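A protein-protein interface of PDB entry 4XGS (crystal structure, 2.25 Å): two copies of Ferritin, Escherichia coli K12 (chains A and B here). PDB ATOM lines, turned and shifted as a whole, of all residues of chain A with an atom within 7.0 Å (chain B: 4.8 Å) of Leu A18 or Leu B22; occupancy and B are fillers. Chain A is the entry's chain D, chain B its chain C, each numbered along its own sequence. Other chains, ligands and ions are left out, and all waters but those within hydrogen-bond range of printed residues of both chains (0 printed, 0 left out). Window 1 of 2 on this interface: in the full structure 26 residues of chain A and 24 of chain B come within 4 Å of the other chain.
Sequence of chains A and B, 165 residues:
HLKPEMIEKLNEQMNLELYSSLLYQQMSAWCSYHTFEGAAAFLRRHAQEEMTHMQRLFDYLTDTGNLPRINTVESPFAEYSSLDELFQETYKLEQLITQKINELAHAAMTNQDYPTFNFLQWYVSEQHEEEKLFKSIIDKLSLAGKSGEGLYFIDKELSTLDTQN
Leu A18 touches Leu B22, but with the chains exchanged Leu A22 does not touch Leu B18 (4.1 Å).
Met B51 touches its own counterpart, Met A51.
Val A73 touches its own counterpart, Val B73.
Of the 8 pairs that touch across the chains among the printed residues, 2 have their exchanged pair printed and touching as well.
Among the printed residues, merely in contact across the chains: Leu A18 with Leu B22, Met A51 with Met B51, Phe A58 with Gln B25, Ile A70 with Leu B22, Ile A70 with Gln B25 and Ile A70 with Pro B76.
Printed residues of chain A within 4 Å of Leu B22: Leu A18 (3.98 Å) and Ile A70 (3.9 Å).
Printed residues of chain B within 4 Å of Val A73: Val B73.
Of the printed residues of chain B, Ile A70 touches Leu B22 (3.9 Å), Gln B25 (3.9 Å), Gln B26 (2.8 Å) and Pro B76 (3.4 Å).
Printed residues of chain A within 4 Å of Pro B76: Ile A70.
Of the printed residues of chain B, Phe A58 touches Gln B25 (3.1 Å).
Of the printed residues of chain A, Gln B25 touches Phe A58 and Ile A70.
Tyr B24 touches none of the printed residues of chain A.
The nearest printed residue of chain B that does not touch Leu A18 is Leu B18 (6.0 Å).
The nearest printed residue of chain A that does not touch Gln B25 is Met A54 (4.3 Å).
The backbone NH (N) of Ile A70 is in hydrogen-bond range of the side-chain amide oxygen (OE1) of Gln B26 (2.8 Å).
N of Val A73 lies within hydrogen-bond range of O of Val B73, at 2.9 Å.
Of the 21 printed residues of chain A, 5 touch a printed residue of chain B.
Printed residues of chain A that touch a printed residue of chain B: Leu A18, Met A51, Phe A58, Ile A70 and Val A73.
Hydrophobic or aromatic side chains of chain A within 4 Å of the printed part of chain B: Leu A18, Met A51, Phe A58 and Ile A70.
Along chain A the printed residues that touch a printed residue of chain B span positions 18 to 73.
Hydrophobic or aromatic side chains of chain B that line the printed part of chain A: Leu B22, Met B51 and Pro B76.
Along chain B the printed residues that touch a printed residue of chain A span positions 22 to 76.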
ATOM      1  N   GLN A  13      18.464  24.650 -21.054  1.00  0.00           N
ATOM      2  CA  GLN A  13      17.929  24.284 -19.740  1.00  0.00           C
ATOM      3  C   GLN A  13      17.379  22.847 -19.790  1.00  0.00           C
ATOM      4  O   GLN A  13      17.590  22.090 -18.852  1.00  0.00           O
ATOM      5  CB  GLN A  13      16.894  25.291 -19.306  1.00  0.00           C
ATOM      6  CG  GLN A  13      16.280  25.017 -17.933  1.00  0.00           C
ATOM      7  CD  GLN A  13      17.273  25.271 -16.853  1.00  0.00           C
ATOM      8  OE1 GLN A  13      18.211  26.049 -17.032  1.00  0.00           O
ATOM      9  NE2 GLN A  13      17.130  24.545 -15.740  1.00  0.00           N
ATOM     10  N   MET A  14      16.701  22.467 -20.880  1.00  0.00           N
ATOM     11  CA  MET A  14      16.302  21.080 -21.044  1.00  0.00           C
ATOM     12  C   MET A  14      17.484  20.140 -20.806  1.00  0.00           C
ATOM     13  O   MET A  14      17.394  19.223 -19.997  1.00  0.00           O
ATOM     14  CB  MET A  14      15.745  20.857 -22.428  1.00  0.00           C
ATOM     15  CG  MET A  14      15.114  19.502 -22.624  1.00  0.00           C
ATOM     16  SD  MET A  14      14.609  19.341 -24.326  1.00  0.00           S
ATOM     17  CE  MET A  14      16.172  19.357 -25.172  1.00  0.00           C
ATOM     18  N   ASN A  15      18.600  20.418 -21.469  1.00  0.00           N
ATOM     19  CA  ASN A  15      19.805  19.631 -21.306  1.00  0.00           C
ATOM     20  C   ASN A  15      20.416  19.636 -19.903  1.00  0.00           C
ATOM     21  O   ASN A  15      20.955  18.617 -19.439  1.00  0.00           O
ATOM     22  CB  ASN A  15      20.894  20.063 -22.356  1.00  0.00           C
ATOM     23  CG  ASN A  15      20.597  19.480 -23.732  1.00  0.00           C
ATOM     24  OD1 ASN A  15      20.975  18.349 -24.024  1.00  0.00           O
ATOM     25  ND2 ASN A  15      19.788  20.187 -24.510  1.00  0.00           N
ATOM     26  N   LEU A  16      20.355  20.786 -19.244  1.00  0.00           N
ATOM     27  CA  LEU A  16      20.831  20.899 -17.883  1.00  0.00           C
ATOM     28  C   LEU A  16      19.941  20.015 -16.989  1.00  0.00           C
ATOM     29  O   LEU A  16      20.455  19.358 -16.057  1.00  0.00           O
ATOM     30  CB  LEU A  16      20.840  22.372 -17.393  1.00  0.00           C
ATOM     31  CG  LEU A  16      21.187  22.613 -15.931  1.00  0.00           C
ATOM     32  CD1 LEU A  16      22.572  22.023 -15.689  1.00  0.00           C
ATOM     33  CD2 LEU A  16      21.135  24.073 -15.562  1.00  0.00           C
ATOM     34  N   GLU A  17      18.630  19.972 -17.247  1.00  0.00           N
ATOM     35  CA  GLU A  17      17.792  19.131 -16.379  1.00  0.00           C
ATOM     36  C   GLU A  17      18.122  17.594 -16.549  1.00  0.00           C
ATOM     37  O   GLU A  17      18.229  16.844 -15.567  1.00  0.00           O
ATOM     38  CB  GLU A  17      16.300  19.374 -16.619  1.00  0.00           C
ATOM     39  CG  GLU A  17      15.808  20.792 -16.373  1.00  0.00           C
ATOM     40  CD  GLU A  17      15.682  21.194 -14.938  1.00  0.00           C
ATOM     41  OE1 GLU A  17      15.581  22.409 -14.650  1.00  0.00           O
ATOM     42  OE2 GLU A  17      15.672  20.298 -14.111  1.00  0.00           O
ATOM     43  N   LEU A  18      18.255  17.185 -17.798  1.00  0.00           N
ATOM     44  CA  LEU A  18      18.702  15.852 -18.204  1.00  0.00           C
ATOM     45  C   LEU A  18      20.031  15.479 -17.510  1.00  0.00           C
ATOM     46  O   LEU A  18      20.151  14.411 -16.855  1.00  0.00           O
ATOM     47  CB  LEU A  18      18.848  15.783 -19.726  1.00  0.00           C
ATOM     48  CG  LEU A  18      19.535  14.531 -20.326  1.00  0.00           C
ATOM     49  CD1 LEU A  18      18.849  13.298 -19.797  1.00  0.00           C
ATOM     50  CD2 LEU A  18      19.462  14.527 -21.860  1.00  0.00           C
ATOM     51  N   TYR A  19      20.978  16.392 -17.578  1.00  0.00           N
ATOM     52  CA  TYR A  19      22.265  16.196 -16.901  1.00  0.00           C
ATOM     53  C   TYR A  19      22.055  16.017 -15.397  1.00  0.00           C
ATOM     54  O   TYR A  19      22.584  15.109 -14.794  1.00  0.00           O
ATOM     55  CB  TYR A  19      23.239  17.368 -17.150  1.00  0.00           C
ATOM     56  CG  TYR A  19      24.508  17.219 -16.305  1.00  0.00           C
ATOM     57  CD1 TYR A  19      25.507  16.377 -16.695  1.00  0.00           C
ATOM     58  CD2 TYR A  19      24.654  17.890 -15.097  1.00  0.00           C
ATOM     59  CE1 TYR A  19      26.665  16.206 -15.926  1.00  0.00           C
ATOM     60  CE2 TYR A  19      25.786  17.737 -14.314  1.00  0.00           C
ATOM     61  CZ  TYR A  19      26.794  16.887 -14.731  1.00  0.00           C
ATOM     62  OH  TYR A  19      27.921  16.740 -13.982  1.00  0.00           O
ATOM     63  N   SER A  20      21.235  16.868 -14.807  1.00  0.00           N
ATOM     64  CA  SER A  20      20.960  16.739 -13.400  1.00  0.00           C
ATOM     65  C   SER A  20      20.368  15.399 -13.049  1.00  0.00           C
ATOM     66  O   SER A  20      20.717  14.816 -11.994  1.00  0.00           O
ATOM     67  CB  SER A  20      20.077  17.886 -12.908  1.00  0.00           C
ATOM     68  OG  SER A  20      20.765  19.088 -13.286  1.00  0.00           O
ATOM     69  N   SER A  21      19.454  14.934 -13.883  1.00  0.00           N
ATOM     70  CA  SER A  21      18.860  13.614 -13.651  1.00  0.00           C
ATOM     71  C   SER A  21      19.965  12.575 -13.555  1.00  0.00           C
ATOM     72  O   SER A  21      19.954  11.724 -12.637  1.00  0.00           O
ATOM     73  CB  SER A  21      17.899  13.203 -14.762  1.00  0.00           C
ATOM     74  OG  SER A  21      17.273  11.965 -14.469  1.00  0.00           O
ATOM     75  N   LEU A  22      20.903  12.638 -14.509  1.00  0.00           N
ATOM     76  CA  LEU A  22      21.913  11.568 -14.642  1.00  0.00           C
ATOM     77  C   LEU A  22      22.957  11.709 -13.546  1.00  0.00           C
ATOM     78  O   LEU A  22      23.529  10.750 -13.106  1.00  0.00           O
ATOM     79  CB  LEU A  22      22.575  11.593 -16.021  1.00  0.00           C
ATOM     80  CG  LEU A  22      21.588  11.365 -17.195  1.00  0.00           C
ATOM     81  CD1 LEU A  22      22.283  11.400 -18.537  1.00  0.00           C
ATOM     82  CD2 LEU A  22      20.910  10.031 -17.086  1.00  0.00           C
ATOM     83  N   LEU A  23      23.206  12.918 -13.117  1.00  0.00           N
ATOM     84  CA  LEU A  23      24.059  13.139 -11.952  1.00  0.00           C
ATOM     85  C   LEU A  23      23.447  12.550 -10.698  1.00  0.00           C
ATOM     86  O   LEU A  23      24.122  11.780 -10.004  1.00  0.00           O
ATOM     87  CB  LEU A  23      24.377  14.608 -11.739  1.00  0.00           C
ATOM     88  CG  LEU A  23      25.371  14.968 -10.613  1.00  0.00           C
ATOM     89  CD1 LEU A  23      26.742  14.327 -10.748  1.00  0.00           C
ATOM     90  CD2 LEU A  23      25.575  16.449 -10.572  1.00  0.00           C
ATOM     91  N   TYR A  24      22.173  12.826 -10.441  1.00  0.00           N
ATOM     92  CA  TYR A  24      21.537  12.216  -9.289  1.00  0.00           C
ATOM     93  C   TYR A  24      21.620  10.699  -9.392  1.00  0.00           C
ATOM     94  O   TYR A  24      21.906  10.021  -8.399  1.00  0.00           O
ATOM     95  CB  TYR A  24      20.100  12.718  -9.064  1.00  0.00           C
ATOM     96  CG  TYR A  24      20.073  14.170  -8.661  1.00  0.00           C
ATOM     97  CD1 TYR A  24      21.215  14.819  -8.183  1.00  0.00           C
ATOM     98  CD2 TYR A  24      18.943  14.925  -8.830  1.00  0.00           C
ATOM     99  CE1 TYR A  24      21.179  16.149  -7.831  1.00  0.00           C
ATOM    100  CE2 TYR A  24      18.892  16.245  -8.476  1.00  0.00           C
ATOM    101  CZ  TYR A  24      20.004  16.854  -7.985  1.00  0.00           C
ATOM    102  OH  TYR A  24      19.916  18.162  -7.631  1.00  0.00           O
ATOM    103  N   ALA A  47      16.300  11.641  -9.337  1.00  0.00           N
ATOM    104  CA  ALA A  47      16.761  11.563 -10.701  1.00  0.00           C
ATOM    105  C   ALA A  47      15.514  11.463 -11.588  1.00  0.00           C
ATOM    106  O   ALA A  47      15.509  12.047 -12.683  1.00  0.00           O
ATOM    107  CB  ALA A  47      17.679  10.336 -10.920  1.00  0.00           C
ATOM    108  N   GLU A  50      13.881  14.899 -11.824  1.00  0.00           N
ATOM    109  CA  GLU A  50      14.532  15.787 -12.756  1.00  0.00           C
ATOM    110  C   GLU A  50      14.260  15.446 -14.218  1.00  0.00           C
ATOM    111  O   GLU A  50      14.181  16.335 -15.017  1.00  0.00           O
ATOM    112  CB  GLU A  50      16.025  15.806 -12.594  1.00  0.00           C
ATOM    113  CG  GLU A  50      16.523  16.315 -11.322  1.00  0.00           C
ATOM    114  CD  GLU A  50      16.183  17.729 -11.061  1.00  0.00           C
ATOM    115  OE1 GLU A  50      15.896  18.535 -12.000  1.00  0.00           O
ATOM    116  OE2 GLU A  50      16.310  18.009  -9.864  1.00  0.00           O
ATOM    117  N   MET A  51      14.176  14.167 -14.547  1.00  0.00           N
ATOM    118  CA  MET A  51      13.702  13.722 -15.822  1.00  0.00           C
ATOM    119  C   MET A  51      12.362  14.337 -16.186  1.00  0.00           C
ATOM    120  O   MET A  51      12.189  14.712 -17.345  1.00  0.00           O
ATOM    121  CB  MET A  51      13.688  12.196 -15.942  1.00  0.00           C
ATOM    122  CG  MET A  51      13.921  11.660 -17.340  1.00  0.00           C
ATOM    123  SD  MET A  51      15.384  12.360 -18.171  1.00  0.00           S
ATOM    124  CE  MET A  51      16.605  11.224 -17.600  1.00  0.00           C
ATOM    125  N   HIS A  53      11.302  17.271 -15.186  1.00  0.00           N
ATOM    126  CA  HIS A  53      11.619  18.644 -15.471  1.00  0.00           C
ATOM    127  C   HIS A  53      12.106  18.817 -16.923  1.00  0.00           C
ATOM    128  O   HIS A  53      11.695  19.733 -17.630  1.00  0.00           O
ATOM    129  CB  HIS A  53      12.653  19.253 -14.488  1.00  0.00           C
ATOM    130  CG  HIS A  53      12.254  19.156 -13.053  1.00  0.00           C
ATOM    131  ND1 HIS A  53      13.080  19.571 -12.031  1.00  0.00           N
ATOM    132  CD2 HIS A  53      11.129  18.691 -12.467  1.00  0.00           C
ATOM    133  CE1 HIS A  53      12.499  19.309 -10.877  1.00  0.00           C
ATOM    134  NE2 HIS A  53      11.318  18.767 -11.109  1.00  0.00           N
ATOM    135  N   MET A  54      12.968  17.920 -17.337  1.00  0.00           N
ATOM    136  CA  MET A  54      13.471  17.842 -18.698  1.00  0.00           C
ATOM    137  C   MET A  54      12.336  17.712 -19.715  1.00  0.00           C
ATOM    138  O   MET A  54      12.283  18.455 -20.669  1.00  0.00           O
ATOM    139  CB  MET A  54      14.416  16.647 -18.789  1.00  0.00           C
ATOM    140  CG  MET A  54      15.172  16.490 -20.102  1.00  0.00           C
ATOM    141  SD  MET A  54      14.144  15.859 -21.462  1.00  0.00           S
ATOM    142  CE  MET A  54      14.049  14.136 -21.040  1.00  0.00           C
ATOM    143  N   PHE A  58      11.020  19.915 -22.949  1.00  0.00           N
ATOM    144  CA  PHE A  58      10.961  19.225 -24.229  1.00  0.00           C
ATOM    145  C   PHE A  58       9.563  19.472 -24.825  1.00  0.00           C
ATOM    146  O   PHE A  58       9.428  19.849 -25.960  1.00  0.00           O
ATOM    147  CB  PHE A  58      11.202  17.724 -23.998  1.00  0.00           C
ATOM    148  CG  PHE A  58      11.588  16.937 -25.227  1.00  0.00           C
ATOM    149  CD1 PHE A  58      10.622  16.427 -26.083  1.00  0.00           C
ATOM    150  CD2 PHE A  58      12.916  16.678 -25.509  1.00  0.00           C
ATOM    151  CE1 PHE A  58      10.981  15.654 -27.201  1.00  0.00           C
ATOM    152  CE2 PHE A  58      13.292  15.938 -26.620  1.00  0.00           C
ATOM    153  CZ  PHE A  58      12.335  15.431 -27.468  1.00  0.00           C
ATOM    154  N   ILE A  70      18.540  17.083 -27.814  1.00  0.00           N
ATOM    155  CA  ILE A  70      19.345  16.504 -26.745  1.00  0.00           C
ATOM    156  C   ILE A  70      20.750  16.481 -27.263  1.00  0.00           C
ATOM    157  O   ILE A  70      21.044  15.778 -28.199  1.00  0.00           O
ATOM    158  CB  ILE A  70      18.865  15.094 -26.376  1.00  0.00           C
ATOM    159  CG1 ILE A  70      17.478  15.210 -25.758  1.00  0.00           C
ATOM    160  CG2 ILE A  70      19.820  14.506 -25.366  1.00  0.00           C
ATOM    161  CD1 ILE A  70      16.777  13.868 -25.662  1.00  0.00           C
ATOM    162  N   ASN A  71      21.599  17.288 -26.648  1.00  0.00           N
ATOM    163  CA  ASN A  71      22.988  17.379 -26.980  1.00  0.00           C
ATOM    164  C   ASN A  71      23.760  16.291 -26.235  1.00  0.00           C
ATOM    165  O   ASN A  71      23.216  15.586 -25.368  1.00  0.00           O
ATOM    166  CB  ASN A  71      23.527  18.746 -26.526  1.00  0.00           C
ATOM    167  CG  ASN A  71      22.883  19.903 -27.260  1.00  0.00           C
ATOM    168  OD1 ASN A  71      22.545  19.825 -28.444  1.00  0.00           O
ATOM    169  ND2 ASN A  71      22.751  21.011 -26.557  1.00  0.00           N
ATOM    170  N   VAL A  73      25.947  14.548 -23.605  1.00  0.00           N
ATOM    171  CA  VAL A  73      25.951  14.713 -22.163  1.00  0.00           C
ATOM    172  C   VAL A  73      27.249  14.139 -21.638  1.00  0.00           C
ATOM    173  O   VAL A  73      27.523  12.969 -21.776  1.00  0.00           O
ATOM    174  CB  VAL A  73      24.818  13.924 -21.505  1.00  0.00           C
ATOM    175  CG1 VAL A  73      24.626  14.419 -20.063  1.00  0.00           C
ATOM    176  CG2 VAL A  73      23.529  13.965 -22.317  1.00  0.00           C
ATOM    177  N   LEU B  18      20.425   3.408 -21.816  1.00  0.00           N
ATOM    178  CA  LEU B  18      20.299   4.860 -21.603  1.00  0.00           C
ATOM    179  C   LEU B  18      20.275   5.614 -22.950  1.00  0.00           C
ATOM    180  O   LEU B  18      19.389   6.438 -23.197  1.00  0.00           O
ATOM    181  CB  LEU B  18      21.421   5.372 -20.694  1.00  0.00           C
ATOM    182  CG  LEU B  18      21.474   6.915 -20.639  1.00  0.00           C
ATOM    183  CD1 LEU B  18      20.173   7.437 -20.130  1.00  0.00           C
ATOM    184  CD2 LEU B  18      22.617   7.409 -19.804  1.00  0.00           C
ATOM    185  N   TYR B  19      21.233   5.302 -23.825  1.00  0.00           N
ATOM    186  CA  TYR B  19      21.250   5.858 -25.189  1.00  0.00           C
ATOM    187  C   TYR B  19      19.912   5.636 -25.910  1.00  0.00           C
ATOM    188  O   TYR B  19      19.324   6.573 -26.458  1.00  0.00           O
ATOM    189  CB  TYR B  19      22.413   5.342 -25.994  1.00  0.00           C
ATOM    190  CG  TYR B  19      22.349   5.818 -27.406  1.00  0.00           C
ATOM    191  CD1 TYR B  19      22.825   7.072 -27.743  1.00  0.00           C
ATOM    192  CD2 TYR B  19      21.785   5.022 -28.421  1.00  0.00           C
ATOM    193  CE1 TYR B  19      22.760   7.551 -29.039  1.00  0.00           C
ATOM    194  CE2 TYR B  19      21.719   5.497 -29.714  1.00  0.00           C
ATOM    195  CZ  TYR B  19      22.196   6.772 -30.007  1.00  0.00           C
ATOM    196  OH  TYR B  19      22.155   7.277 -31.284  1.00  0.00           O
ATOM    197  N   SER B  20      19.398   4.433 -25.831  1.00  0.00           N
ATOM    198  CA  SER B  20      18.148   4.076 -26.543  1.00  0.00           C
ATOM    199  C   SER B  20      16.960   4.862 -26.016  1.00  0.00           C
ATOM    200  O   SER B  20      16.067   5.270 -26.794  1.00  0.00           O
ATOM    201  CB  SER B  20      17.860   2.579 -26.424  1.00  0.00           C
ATOM    202  OG  SER B  20      18.973   1.843 -26.957  1.00  0.00           O
ATOM    203  N   SER B  21      16.934   5.063 -24.703  1.00  0.00           N
ATOM    204  CA  SER B  21      15.943   5.942 -24.110  1.00  0.00           C
ATOM    205  C   SER B  21      16.020   7.327 -24.807  1.00  0.00           C
ATOM    206  O   SER B  21      14.995   7.848 -25.306  1.00  0.00           O
ATOM    207  CB  SER B  21      16.120   6.081 -22.616  1.00  0.00           C
ATOM    208  OG  SER B  21      15.049   6.810 -22.056  1.00  0.00           O
ATOM    209  N   LEU B  22      17.211   7.910 -24.841  1.00  0.00           N
ATOM    210  CA  LEU B  22      17.324   9.262 -25.302  1.00  0.00           C
ATOM    211  C   LEU B  22      17.052   9.348 -26.781  1.00  0.00           C
ATOM    212  O   LEU B  22      16.504  10.323 -27.258  1.00  0.00           O
ATOM    213  CB  LEU B  22      18.684   9.864 -24.964  1.00  0.00           C
ATOM    214  CG  LEU B  22      18.911   9.865 -23.413  1.00  0.00           C
ATOM    215  CD1 LEU B  22      20.294  10.358 -23.123  1.00  0.00           C
ATOM    216  CD2 LEU B  22      17.906  10.730 -22.693  1.00  0.00           C
ATOM    217  N   LEU B  23      17.403   8.309 -27.510  1.00  0.00           N
ATOM    218  CA  LEU B  23      17.096   8.269 -28.908  1.00  0.00           C
ATOM    219  C   LEU B  23      15.596   8.225 -29.149  1.00  0.00           C
ATOM    220  O   LEU B  23      15.069   8.952 -30.020  1.00  0.00           O
ATOM    221  CB  LEU B  23      17.815   7.110 -29.607  1.00  0.00           C
ATOM    222  CG  LEU B  23      17.496   6.954 -31.096  1.00  0.00           C
ATOM    223  CD1 LEU B  23      18.125   8.100 -31.873  1.00  0.00           C
ATOM    224  CD2 LEU B  23      17.949   5.603 -31.604  1.00  0.00           C
ATOM    225  N   TYR B  24      14.881   7.420 -28.377  1.00  0.00           N
ATOM    226  CA  TYR B  24      13.405   7.379 -28.548  1.00  0.00           C
ATOM    227  C   TYR B  24      12.812   8.730 -28.205  1.00  0.00           C
ATOM    228  O   TYR B  24      11.858   9.189 -28.871  1.00  0.00           O
ATOM    229  CB  TYR B  24      12.702   6.225 -27.797  1.00  0.00           C
ATOM    230  CG  TYR B  24      13.075   4.856 -28.320  1.00  0.00           C
ATOM    231  CD1 TYR B  24      13.488   4.679 -29.623  1.00  0.00           C
ATOM    232  CD2 TYR B  24      13.122   3.753 -27.494  1.00  0.00           C
ATOM    233  CE1 TYR B  24      13.877   3.435 -30.090  1.00  0.00           C
ATOM    234  CE2 TYR B  24      13.517   2.513 -27.957  1.00  0.00           C
ATOM    235  CZ  TYR B  24      13.865   2.362 -29.260  1.00  0.00           C
ATOM    236  OH  TYR B  24      14.227   1.171 -29.772  1.00  0.00           O
ATOM    237  N   GLN B  25      13.378   9.370 -27.182  1.00  0.00           N
ATOM    238  CA  GLN B  25      12.922  10.700 -26.801  1.00  0.00           C
ATOM    239  C   GLN B  25      13.196  11.703 -27.963  1.00  0.00           C
ATOM    240  O   GLN B  25      12.315  12.442 -28.341  1.00  0.00           O
ATOM    241  CB  GLN B  25      13.658  11.138 -25.561  1.00  0.00           C
ATOM    242  CG  GLN B  25      13.158  12.449 -25.009  1.00  0.00           C
ATOM    243  CD  GLN B  25      11.839  12.333 -24.301  1.00  0.00           C
ATOM    244  OE1 GLN B  25      11.551  11.319 -23.709  1.00  0.00           O
ATOM    245  NE2 GLN B  25      11.030  13.347 -24.409  1.00  0.00           N
ATOM    246  N   GLN B  26      14.415  11.711 -28.510  1.00  0.00           N
ATOM    247  CA  GLN B  26      14.740  12.573 -29.603  1.00  0.00           C
ATOM    248  C   GLN B  26      13.841  12.294 -30.838  1.00  0.00           C
ATOM    249  O   GLN B  26      13.328  13.219 -31.472  1.00  0.00           O
ATOM    250  CB  GLN B  26      16.174  12.411 -29.981  1.00  0.00           C
ATOM    251  CG  GLN B  26      16.677  13.463 -30.987  1.00  0.00           C
ATOM    252  CD  GLN B  26      16.589  14.886 -30.402  1.00  0.00           C
ATOM    253  OE1 GLN B  26      17.263  15.235 -29.416  1.00  0.00           O
ATOM    254  NE2 GLN B  26      15.733  15.686 -30.985  1.00  0.00           N
ATOM    255  N   MET B  51      14.402   3.476 -20.114  1.00  0.00           N
ATOM    256  CA  MET B  51      14.981   3.899 -18.877  1.00  0.00           C
ATOM    257  C   MET B  51      14.865   2.874 -17.741  1.00  0.00           C
ATOM    258  O   MET B  51      15.827   2.732 -16.918  1.00  0.00           O
ATOM    259  CB  MET B  51      14.418   5.261 -18.428  1.00  0.00           C
ATOM    260  CG  MET B  51      15.424   6.013 -17.596  1.00  0.00           C
ATOM    261  SD  MET B  51      16.954   6.467 -18.414  1.00  0.00           S
ATOM    262  CE  MET B  51      16.342   7.738 -19.438  1.00  0.00           C
ATOM    263  N   VAL B  73      27.260  10.445 -23.245  1.00  0.00           N
ATOM    264  CA  VAL B  73      26.269   9.993 -24.159  1.00  0.00           C
ATOM    265  C   VAL B  73      26.256  10.930 -25.327  1.00  0.00           C
ATOM    266  O   VAL B  73      25.920  12.103 -25.173  1.00  0.00           O
ATOM    267  CB  VAL B  73      24.840  10.119 -23.579  1.00  0.00           C
ATOM    268  CG1 VAL B  73      23.858   9.338 -24.489  1.00  0.00           C
ATOM    269  CG2 VAL B  73      24.785   9.625 -22.159  1.00  0.00           C
ATOM    270  N   PRO B  76      21.785  12.009 -29.509  1.00  0.00           N
ATOM    271  CA  PRO B  76      20.961  11.239 -30.415  1.00  0.00           C
ATOM    272  C   PRO B  76      20.379  11.983 -31.636  1.00  0.00           C
ATOM    273  O   PRO B  76      19.618  11.371 -32.393  1.00  0.00           O
ATOM    274  CB  PRO B  76      19.790  10.805 -29.514  1.00  0.00           C
ATOM    275  CG  PRO B  76      19.669  11.868 -28.511  1.00  0.00           C
ATOM    276  CD  PRO B  76      21.074  12.343 -28.267  1.00  0.00           C
